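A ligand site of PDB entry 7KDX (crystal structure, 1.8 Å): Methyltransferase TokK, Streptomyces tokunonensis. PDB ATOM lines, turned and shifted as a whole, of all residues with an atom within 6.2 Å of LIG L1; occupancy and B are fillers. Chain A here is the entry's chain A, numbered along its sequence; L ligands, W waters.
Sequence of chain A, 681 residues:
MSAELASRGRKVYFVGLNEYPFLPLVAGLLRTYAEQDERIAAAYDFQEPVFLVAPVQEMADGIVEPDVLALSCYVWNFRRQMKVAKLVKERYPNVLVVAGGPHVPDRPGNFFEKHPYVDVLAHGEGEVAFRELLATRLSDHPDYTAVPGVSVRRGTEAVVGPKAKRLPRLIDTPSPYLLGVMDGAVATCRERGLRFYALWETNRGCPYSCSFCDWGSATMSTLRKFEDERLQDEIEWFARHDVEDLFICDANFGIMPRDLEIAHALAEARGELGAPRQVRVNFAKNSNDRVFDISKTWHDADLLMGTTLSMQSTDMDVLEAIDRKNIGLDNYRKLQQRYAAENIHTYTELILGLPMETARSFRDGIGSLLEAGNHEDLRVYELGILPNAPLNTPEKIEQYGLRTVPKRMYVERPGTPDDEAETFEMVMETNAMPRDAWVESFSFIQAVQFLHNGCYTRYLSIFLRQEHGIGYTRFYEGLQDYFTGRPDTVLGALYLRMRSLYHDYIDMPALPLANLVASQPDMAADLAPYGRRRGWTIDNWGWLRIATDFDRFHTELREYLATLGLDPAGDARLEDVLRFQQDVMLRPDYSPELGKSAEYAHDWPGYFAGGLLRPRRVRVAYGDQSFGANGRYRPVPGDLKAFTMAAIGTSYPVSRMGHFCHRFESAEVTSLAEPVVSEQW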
ATOM      1  N   CYS A 206     -18.267 -17.551  16.802  1.00  0.00           N
ATOM      2  CA  CYS A 206     -17.245 -16.939  17.639  1.00  0.00           C
ATOM      3  C   CYS A 206     -17.949 -15.953  18.563  1.00  0.00           C
ATOM      4  O   CYS A 206     -18.750 -15.132  18.087  1.00  0.00           O
ATOM      5  CB  CYS A 206     -16.178 -16.197  16.819  1.00  0.00           C
ATOM      6  SG  CYS A 206     -14.971 -15.325  17.883  1.00  0.00           S
ATOM      7  N   TYR A 208     -16.717 -13.421  20.062  1.00  0.00           N
ATOM      8  CA  TYR A 208     -16.060 -12.126  20.072  1.00  0.00           C
ATOM      9  C   TYR A 208     -16.511 -11.324  18.854  1.00  0.00           C
ATOM     10  O   TYR A 208     -17.478 -11.682  18.172  1.00  0.00           O
ATOM     11  CB  TYR A 208     -14.548 -12.332  20.168  1.00  0.00           C
ATOM     12  CG  TYR A 208     -14.213 -13.299  21.285  1.00  0.00           C
ATOM     13  CD1 TYR A 208     -14.595 -13.029  22.600  1.00  0.00           C
ATOM     14  CD2 TYR A 208     -13.570 -14.509  21.022  1.00  0.00           C
ATOM     15  CE1 TYR A 208     -14.320 -13.916  23.617  1.00  0.00           C
ATOM     16  CE2 TYR A 208     -13.281 -15.397  22.053  1.00  0.00           C
ATOM     17  CZ  TYR A 208     -13.661 -15.089  23.342  1.00  0.00           C
ATOM     18  OH  TYR A 208     -13.387 -15.976  24.359  1.00  0.00           O
ATOM     19  N   CYS A 210     -14.240  -9.032  16.573  1.00  0.00           N
ATOM     20  CA  CYS A 210     -13.211  -8.323  15.814  1.00  0.00           C
ATOM     21  C   CYS A 210     -13.783  -7.814  14.485  1.00  0.00           C
ATOM     22  O   CYS A 210     -14.338  -8.594  13.709  1.00  0.00           O
ATOM     23  CB  CYS A 210     -12.018  -9.251  15.568  1.00  0.00           C
ATOM     24  SG  CYS A 210     -11.382 -10.004  17.073  1.00  0.00           S
ATOM     25  N   PHE A 212     -12.748  -6.773  11.600  1.00  0.00           N
ATOM     26  CA  PHE A 212     -12.274  -7.216  10.289  1.00  0.00           C
ATOM     27  C   PHE A 212     -12.766  -8.613   9.914  1.00  0.00           C
ATOM     28  O   PHE A 212     -12.620  -9.018   8.755  1.00  0.00           O
ATOM     29  CB  PHE A 212     -10.744  -7.213  10.252  1.00  0.00           C
ATOM     30  CG  PHE A 212     -10.109  -8.050  11.331  1.00  0.00           C
ATOM     31  CD1 PHE A 212      -9.995  -9.425  11.182  1.00  0.00           C
ATOM     32  CD2 PHE A 212      -9.661  -7.465  12.509  1.00  0.00           C
ATOM     33  CE1 PHE A 212      -9.441 -10.197  12.180  1.00  0.00           C
ATOM     34  CE2 PHE A 212      -9.107  -8.237  13.506  1.00  0.00           C
ATOM     35  CZ  PHE A 212      -8.994  -9.604  13.346  1.00  0.00           C
ATOM     36  N   CYS A 213     -13.318  -9.365  10.863  1.00  0.00           N
ATOM     37  CA  CYS A 213     -13.513 -10.806  10.755  1.00  0.00           C
ATOM     38  C   CYS A 213     -14.951 -11.141  10.389  1.00  0.00           C
ATOM     39  O   CYS A 213     -15.891 -10.410  10.705  1.00  0.00           O
ATOM     40  CB  CYS A 213     -13.136 -11.473  12.086  1.00  0.00           C
ATOM     41  SG  CYS A 213     -12.994 -13.265  12.075  1.00  0.00           S
ATOM     42  N   TRP A 215     -15.776 -14.832  10.585  1.00  0.00           N
ATOM     43  CA  TRP A 215     -15.514 -16.260  10.761  1.00  0.00           C
ATOM     44  C   TRP A 215     -16.800 -17.069  10.754  1.00  0.00           C
ATOM     45  O   TRP A 215     -17.659 -16.890  11.627  1.00  0.00           O
ATOM     46  CB  TRP A 215     -14.767 -16.487  12.063  1.00  0.00           C
ATOM     47  CG  TRP A 215     -14.018 -17.776  12.121  1.00  0.00           C
ATOM     48  CD1 TRP A 215     -14.425 -18.947  12.676  1.00  0.00           C
ATOM     49  CD2 TRP A 215     -12.711 -18.009  11.591  1.00  0.00           C
ATOM     50  NE1 TRP A 215     -13.451 -19.905  12.526  1.00  0.00           N
ATOM     51  CE2 TRP A 215     -12.393 -19.353  11.861  1.00  0.00           C
ATOM     52  CE3 TRP A 215     -11.781 -17.225  10.907  1.00  0.00           C
ATOM     53  CZ2 TRP A 215     -11.180 -19.923  11.482  1.00  0.00           C
ATOM     54  CZ3 TRP A 215     -10.586 -17.786  10.518  1.00  0.00           C
ATOM     55  CH2 TRP A 215     -10.300 -19.124  10.807  1.00  0.00           C
ATOM     56  N   ASP A 250     -13.165 -24.561  13.802  1.00  0.00           N
ATOM     57  CA  ASP A 250     -13.552 -23.812  14.994  1.00  0.00           C
ATOM     58  C   ASP A 250     -12.812 -22.477  15.083  1.00  0.00           C
ATOM     59  O   ASP A 250     -11.639 -22.365  14.718  1.00  0.00           O
ATOM     60  CB  ASP A 250     -13.275 -24.626  16.253  1.00  0.00           C
ATOM     61  CG  ASP A 250     -14.062 -25.923  16.312  1.00  0.00           C
ATOM     62  OD1 ASP A 250     -14.769 -26.270  15.339  1.00  0.00           O
ATOM     63  OD2 ASP A 250     -13.973 -26.602  17.362  1.00  0.00           O
ATOM     64  N   ALA A 251     -13.512 -21.465  15.615  1.00  0.00           N
ATOM     65  CA  ALA A 251     -12.887 -20.156  15.797  1.00  0.00           C
ATOM     66  C   ALA A 251     -11.906 -20.144  16.957  1.00  0.00           C
ATOM     67  O   ALA A 251     -10.904 -19.422  16.907  1.00  0.00           O
ATOM     68  CB  ALA A 251     -13.959 -19.087  16.013  1.00  0.00           C
ATOM     69  N   ASN A 252     -12.172 -20.927  18.018  1.00  0.00           N
ATOM     70  CA  ASN A 252     -11.433 -20.796  19.269  1.00  0.00           C
ATOM     71  C   ASN A 252     -11.246 -22.168  19.913  1.00  0.00           C
ATOM     72  O   ASN A 252     -11.764 -22.442  20.994  1.00  0.00           O
ATOM     73  CB  ASN A 252     -12.159 -19.857  20.251  1.00  0.00           C
ATOM     74  CG  ASN A 252     -12.165 -18.421  19.801  1.00  0.00           C
ATOM     75  OD1 ASN A 252     -11.175 -17.704  19.985  1.00  0.00           O
ATOM     76  ND2 ASN A 252     -13.272 -17.981  19.229  1.00  0.00           N
ATOM     77  N   ASN A 282      -7.454 -23.168  14.558  1.00  0.00           N
ATOM     78  CA  ASN A 282      -7.206 -21.903  15.224  1.00  0.00           C
ATOM     79  C   ASN A 282      -7.534 -22.053  16.706  1.00  0.00           C
ATOM     80  O   ASN A 282      -8.648 -22.456  17.065  1.00  0.00           O
ATOM     81  CB  ASN A 282      -8.062 -20.805  14.593  1.00  0.00           C
ATOM     82  CG  ASN A 282      -7.503 -20.369  13.256  1.00  0.00           C
ATOM     83  OD1 ASN A 282      -6.663 -19.479  13.199  1.00  0.00           O
ATOM     84  ND2 ASN A 282      -7.973 -21.005  12.177  1.00  0.00           N
ATOM     85  N   PHE A 283      -6.554 -21.753  17.563  1.00  0.00           N
ATOM     86  CA  PHE A 283      -6.719 -21.896  19.001  1.00  0.00           C
ATOM     87  C   PHE A 283      -7.289 -20.620  19.632  1.00  0.00           C
ATOM     88  O   PHE A 283      -7.143 -19.522  19.096  1.00  0.00           O
ATOM     89  CB  PHE A 283      -5.383 -22.249  19.653  1.00  0.00           C
ATOM     90  CG  PHE A 283      -4.968 -23.684  19.445  1.00  0.00           C
ATOM     91  CD1 PHE A 283      -5.393 -24.676  20.330  1.00  0.00           C
ATOM     92  CD2 PHE A 283      -4.166 -24.050  18.370  1.00  0.00           C
ATOM     93  CE1 PHE A 283      -5.019 -25.998  20.147  1.00  0.00           C
ATOM     94  CE2 PHE A 283      -3.788 -25.379  18.181  1.00  0.00           C
ATOM     95  CZ  PHE A 283      -4.212 -26.342  19.068  1.00  0.00           C
ATOM     96  N   ALA A 284      -7.905 -20.791  20.790  1.00  0.00           N
ATOM     97  CA  ALA A 284      -8.777 -19.773  21.377  1.00  0.00           C
ATOM     98  C   ALA A 284      -8.041 -18.458  21.635  1.00  0.00           C
ATOM     99  O   ALA A 284      -6.880 -18.439  22.051  1.00  0.00           O
ATOM    100  CB  ALA A 284      -9.382 -20.290  22.682  1.00  0.00           C
ATOM    101  N   LYS A 285      -8.750 -17.347  21.394  1.00  0.00           N
ATOM    102  CA  LYS A 285      -8.184 -16.021  21.648  1.00  0.00           C
ATOM    103  C   LYS A 285      -7.782 -15.854  23.103  1.00  0.00           C
ATOM    104  O   LYS A 285      -6.672 -15.399  23.407  1.00  0.00           O
ATOM    105  CB  LYS A 285      -9.202 -14.939  21.257  1.00  0.00           C
ATOM    106  CG  LYS A 285      -8.660 -13.512  21.420  1.00  0.00           C
ATOM    107  CD  LYS A 285      -9.668 -12.458  20.945  1.00  0.00           C
ATOM    108  CE  LYS A 285     -10.849 -12.320  21.888  1.00  0.00           C
ATOM    109  NZ  LYS A 285     -10.455 -11.759  23.212  1.00  0.00           N
ATOM    110  N   ASN A 286      -8.669 -16.198  24.030  1.00  0.00           N
ATOM    111  CA  ASN A 286      -8.360 -16.105  25.454  1.00  0.00           C
ATOM    112  C   ASN A 286      -7.645 -17.393  25.865  1.00  0.00           C
ATOM    113  O   ASN A 286      -8.216 -18.308  26.467  1.00  0.00           O
ATOM    114  CB  ASN A 286      -9.629 -15.854  26.270  1.00  0.00           C
ATOM    115  CG  ASN A 286     -10.319 -14.566  25.864  1.00  0.00           C
ATOM    116  OD1 ASN A 286      -9.743 -13.735  25.150  1.00  0.00           O
ATOM    117  ND2 ASN A 286     -11.553 -14.366  26.335  1.00  0.00           N
ATOM    118  N   THR A 308      -2.010 -21.161  18.171  1.00  0.00           N
ATOM    119  CA  THR A 308      -2.356 -19.782  17.833  1.00  0.00           C
ATOM    120  C   THR A 308      -2.326 -18.899  19.070  1.00  0.00           C
ATOM    121  O   THR A 308      -3.085 -19.127  20.025  1.00  0.00           O
ATOM    122  CB  THR A 308      -3.736 -19.719  17.191  1.00  0.00           C
ATOM    123  OG1 THR A 308      -3.944 -20.857  16.348  1.00  0.00           O
ATOM    124  CG2 THR A 308      -3.870 -18.448  16.373  1.00  0.00           C
ATOM    125  N   LEU A 309      -1.472 -17.870  19.056  1.00  0.00           N
ATOM    126  CA  LEU A 309      -1.479 -16.818  20.069  1.00  0.00           C
ATOM    127  C   LEU A 309      -1.513 -15.460  19.359  1.00  0.00           C
ATOM    128  O   LEU A 309      -0.581 -14.674  19.425  1.00  0.00           O
ATOM    129  CB  LEU A 309      -0.272 -16.900  21.000  1.00  0.00           C
ATOM    130  CG  LEU A 309      -0.156 -18.166  21.850  1.00  0.00           C
ATOM    131  CD1 LEU A 309       1.163 -18.174  22.626  1.00  0.00           C
ATOM    132  CD2 LEU A 309      -1.350 -18.274  22.777  1.00  0.00           C
ATOM    133  N   SER A 310      -2.615 -15.215  18.650  1.00  0.00           N
ATOM    134  CA  SER A 310      -2.628 -14.100  17.713  1.00  0.00           C
ATOM    135  C   SER A 310      -3.104 -12.815  18.381  1.00  0.00           C
ATOM    136  O   SER A 310      -3.771 -12.827  19.424  1.00  0.00           O
ATOM    137  CB  SER A 310      -3.509 -14.453  16.517  1.00  0.00           C
ATOM    138  OG  SER A 310      -2.818 -15.361  15.685  1.00  0.00           O
ATOM    139  N   MET A 311      -2.717 -11.697  17.782  1.00  0.00           N
ATOM    140  CA  MET A 311      -2.878 -10.347  18.322  1.00  0.00           C
ATOM    141  C   MET A 311      -3.591  -9.404  17.371  1.00  0.00           C
ATOM    142  O   MET A 311      -4.362  -8.547  17.830  1.00  0.00           O
ATOM    143  CB  MET A 311      -1.501  -9.772  18.647  1.00  0.00           C
ATOM    144  CG  MET A 311      -0.785 -10.469  19.788  1.00  0.00           C
ATOM    145  SD  MET A 311      -1.572 -10.037  21.344  1.00  0.00           S
ATOM    146  CE  MET A 311      -0.535 -10.928  22.503  1.00  0.00           C
ATOM    147  N   GLN A 312      -3.341  -9.522  16.060  1.00  0.00           N
ATOM    148  CA  GLN A 312      -3.788  -8.607  15.017  1.00  0.00           C
ATOM    149  C   GLN A 312      -3.092  -7.261  15.163  1.00  0.00           C
ATOM    150  O   GLN A 312      -2.525  -6.741  14.187  1.00  0.00           O
ATOM    151  CB  GLN A 312      -5.321  -8.451  15.019  1.00  0.00           C
ATOM    152  CG  GLN A 312      -6.123  -9.711  15.402  1.00  0.00           C
ATOM    153  CD  GLN A 312      -5.820 -10.926  14.547  1.00  0.00           C
ATOM    154  OE1 GLN A 312      -5.091 -10.857  13.562  1.00  0.00           O
ATOM    155  NE2 GLN A 312      -6.399 -12.063  14.924  1.00  0.00           N
ATOM    156  N   ARG A 324     -11.458  -5.494  19.809  1.00  0.00           N
ATOM    157  CA  ARG A 324     -10.717  -6.682  20.192  1.00  0.00           C
ATOM    158  C   ARG A 324      -9.944  -6.425  21.466  1.00  0.00           C
ATOM    159  O   ARG A 324      -9.277  -5.390  21.605  1.00  0.00           O
ATOM    160  CB  ARG A 324      -9.760  -7.119  19.070  1.00  0.00           C
ATOM    161  CG  ARG A 324      -8.977  -8.377  19.432  1.00  0.00           C
ATOM    162  CD  ARG A 324      -8.048  -8.806  18.312  1.00  0.00           C
ATOM    163  NE  ARG A 324      -7.220  -9.942  18.727  1.00  0.00           N
ATOM    164  CZ  ARG A 324      -7.430 -11.204  18.346  1.00  0.00           C
ATOM    165  NH1 ARG A 324      -8.427 -11.507  17.533  1.00  0.00           N
ATOM    166  NH2 ARG A 324      -6.624 -12.157  18.790  1.00  0.00           N
ATOM    167  N   ASN A 326      -6.927  -8.178  23.717  1.00  0.00           N
ATOM    168  CA  ASN A 326      -5.854  -9.163  23.691  1.00  0.00           C
ATOM    169  C   ASN A 326      -5.396  -9.491  25.094  1.00  0.00           C
ATOM    170  O   ASN A 326      -5.614  -8.741  26.054  1.00  0.00           O
ATOM    171  CB  ASN A 326      -4.661  -8.660  22.877  1.00  0.00           C
ATOM    172  CG  ASN A 326      -4.829  -8.851  21.390  1.00  0.00           C
ATOM    173  OD1 ASN A 326      -5.476  -9.805  20.948  1.00  0.00           O
ATOM    174  ND2 ASN A 326      -4.233  -7.965  20.608  1.00  0.00           N
ATOM    175  N   GLU A 349      -0.270 -13.908  14.785  1.00  0.00           N
ATOM    176  CA  GLU A 349      -0.676 -13.221  13.567  1.00  0.00           C
ATOM    177  C   GLU A 349      -0.907 -11.738  13.826  1.00  0.00           C
ATOM    178  O   GLU A 349      -1.433 -11.356  14.874  1.00  0.00           O
ATOM    179  CB  GLU A 349      -1.942 -13.840  12.977  1.00  0.00           C
ATOM    180  CG  GLU A 349      -1.739 -15.225  12.408  1.00  0.00           C
ATOM    181  CD  GLU A 349      -3.013 -16.024  12.363  1.00  0.00           C
ATOM    182  OE1 GLU A 349      -3.801 -15.954  13.323  1.00  0.00           O
ATOM    183  OE2 GLU A 349      -3.223 -16.729  11.347  1.00  0.00           O
HETATM  184  N1  LIG L   1     -10.036 -16.557  17.429  1.00  0.00           N
HETATM  185  C1  LIG L   1      -8.598 -16.646  17.679  1.00  0.00           C
HETATM  186  C2  LIG L   1      -8.000 -15.253  17.715  1.00  0.00           C
HETATM  187  O1  LIG L   1      -8.550 -14.321  17.107  1.00  0.00           O
HETATM  188  C3  LIG L   1      -7.896 -17.485  16.606  1.00  0.00           C
HETATM  189  C4  LIG L   1      -7.576 -16.720  15.324  1.00  0.00           C
HETATM  190  S1  LIG L   1      -9.015 -16.128  14.393  1.00  0.00           S
HETATM  191  C5  LIG L   1      -9.834 -17.687  14.035  1.00  0.00           C
HETATM  192  O2  LIG L   1      -6.967 -15.014  18.348  1.00  0.00           O
HETATM  193 FE1  LG2 L   2     -11.753 -12.206  16.452  1.00  0.00          FE
HETATM  194 FE2  LG2 L   2     -13.379 -14.372  16.651  1.00  0.00          FE
HETATM  195 FE3  LG2 L   2     -10.626 -14.733  16.080  1.00  0.00          FE
HETATM  196 FE4  LG2 L   2     -12.392 -13.636  14.211  1.00  0.00          FE
HETATM  197  S1  LG2 L   2     -12.452 -15.739  15.027  1.00  0.00           S
HETATM  198  S2  LG2 L   2     -10.292 -12.867  14.780  1.00  0.00           S
HETATM  199  S3  LG2 L   2     -13.836 -12.452  15.561  1.00  0.00           S
HETATM  200  S4  LG2 L   2     -11.617 -13.831  18.022  1.00  0.00           S
HETATM  201  N1  LG3 L   3      -7.965  -9.599   6.527  1.00  0.00           N
HETATM  202  C1  LG3 L   3      -6.773 -10.120   6.854  1.00  0.00           C
HETATM  203  N2  LG3 L   3      -6.497 -11.088   7.736  1.00  0.00           N
HETATM  204  C2  LG3 L   3      -7.607 -11.553   8.321  1.00  0.00           C
HETATM  205  N3  LG3 L   3      -7.704 -12.550   9.251  1.00  0.00           N
HETATM  206  C3  LG3 L   3      -9.043 -12.678   9.523  1.00  0.00           C
HETATM  207  N4  LG3 L   3      -9.803 -11.850   8.855  1.00  0.00           N
HETATM  208  C4  LG3 L   3      -8.904 -11.122   8.084  1.00  0.00           C
HETATM  209  C5  LG3 L   3      -9.071 -10.088   7.146  1.00  0.00           C
HETATM  210  N5  LG3 L   3     -10.267  -9.564   6.865  1.00  0.00           N
HETATM  211  C6  LG3 L   3      -6.613 -13.298   9.860  1.00  0.00           C
HETATM  212  C7  LG3 L   3      -6.380 -12.966  11.341  1.00  0.00           C
HETATM  213  C8  LG3 L   3      -6.858 -14.239  12.052  1.00  0.00           C
HETATM  214  C9  LG3 L   3      -6.515 -15.299  11.022  1.00  0.00           C
HETATM  215  C10 LG3 L   3      -7.240 -16.620  11.185  1.00  0.00           C
HETATM  216  O1  LG3 L   3      -6.898 -14.688   9.773  1.00  0.00           O
HETATM  217  O2  LG3 L   3      -4.996 -12.701  11.543  1.00  0.00           O
HETATM  218  O3  LG3 L   3      -6.182 -14.493  13.267  1.00  0.00           O
HETATM  219  O   HOH W   1      -5.163 -16.803  19.298  1.00  0.00           O
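Water W1 lies within hydrogen-bond range of O2 of LIG L1 (2.7 Å), N of Ser 310 (3.1 Å), O of Thr 308 (3.2 Å) and O of Phe 283 (3.4 Å).
Merely in contact with LIG L1: Trp 215, Asn 282, Phe 283, Lys 285, Ser 310 and Gln 312. Hydrophobic or aromatic side chains within 4 Å of LIG L1: Trp 215. Of the 22 residues printed, 9 come within 4 Å of LIG L1. The nearest printed residue that does not touch LIG L1 is Thr 308 (4.1 Å).
N1 of LIG L1 is bound to FE3 of LG2 L2, 2.3 Å away. S1 of LIG L1 lies close to O3 of LG3 L3.
NH2 of Arg 324 is in salt-bridge range of O2 of LIG L1, at 2.9 Å. OD1 of Asn 252 lies close to N1 of LIG L1 (3.0 Å). The backbone carbonyl oxygen (O) of Ala 251 lies close to a nitrogen (N1) of LIG L1, 3.0 Å away. S2 of LG2 L2 sits close to NH1 of Arg 324 (3.6 Å). SG of Cys 206 binds FE2 of LG2 L2, 2.2 Å away. A sulfur (S3) of LG2 L2 sits close to the backbone NH (N) of Cys 210 (3.6 Å). The side-chain sulfur of Cys 210 binds an iron atom (FE1) of LG2 L2 (2.3 Å). FE4 of LG2 L2 is bound by SG of Cys 213 (2.3 Å). OE1 of Gln 312 lies within hydrogen-bond range of O2 of LG3 L3, at 2.7 Å. O3 of LG3 L3 sits at hydrogen-bond distance from OE1 of Glu 349, 2.8 Å away. The backbone carbonyl oxygen (O) of Phe 212 is in hydrogen-bond range of a nitrogen (N5) of LG3 L3.
The side-chain amide nitrogen of Gln 312 sits close to the guanidinium group of Arg 324 (3.4 Å). The guanidinium group of Arg 324 lies close to the side-chain sulfur of Cys 210, at 3.3 Å. The guanidinium group of Arg 324 lies within hydrogen-bond range of the side-chain amide oxygen of Asn 326, at 2.8 Å. The side-chain hydroxyl (OG1) of Thr 308 sits at hydrogen-bond distance from the backbone NH (N) of Phe 283 (3.0 Å). N of Trp 215 lies close to SG of Cys 213. The side-chain amino group (NZ) of Lys 285 is in hydrogen-bond range of the side-chain amide oxygen (OD1) of Asn 286 (2.9 Å). The backbone NH (N) of Gln 312 sits at hydrogen-bond distance from the backbone carbonyl oxygen (O) of Glu 349. The side-chain hydroxyl of Ser 310 is in hydrogen-bond range of the side-chain carboxylate of Glu 349.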
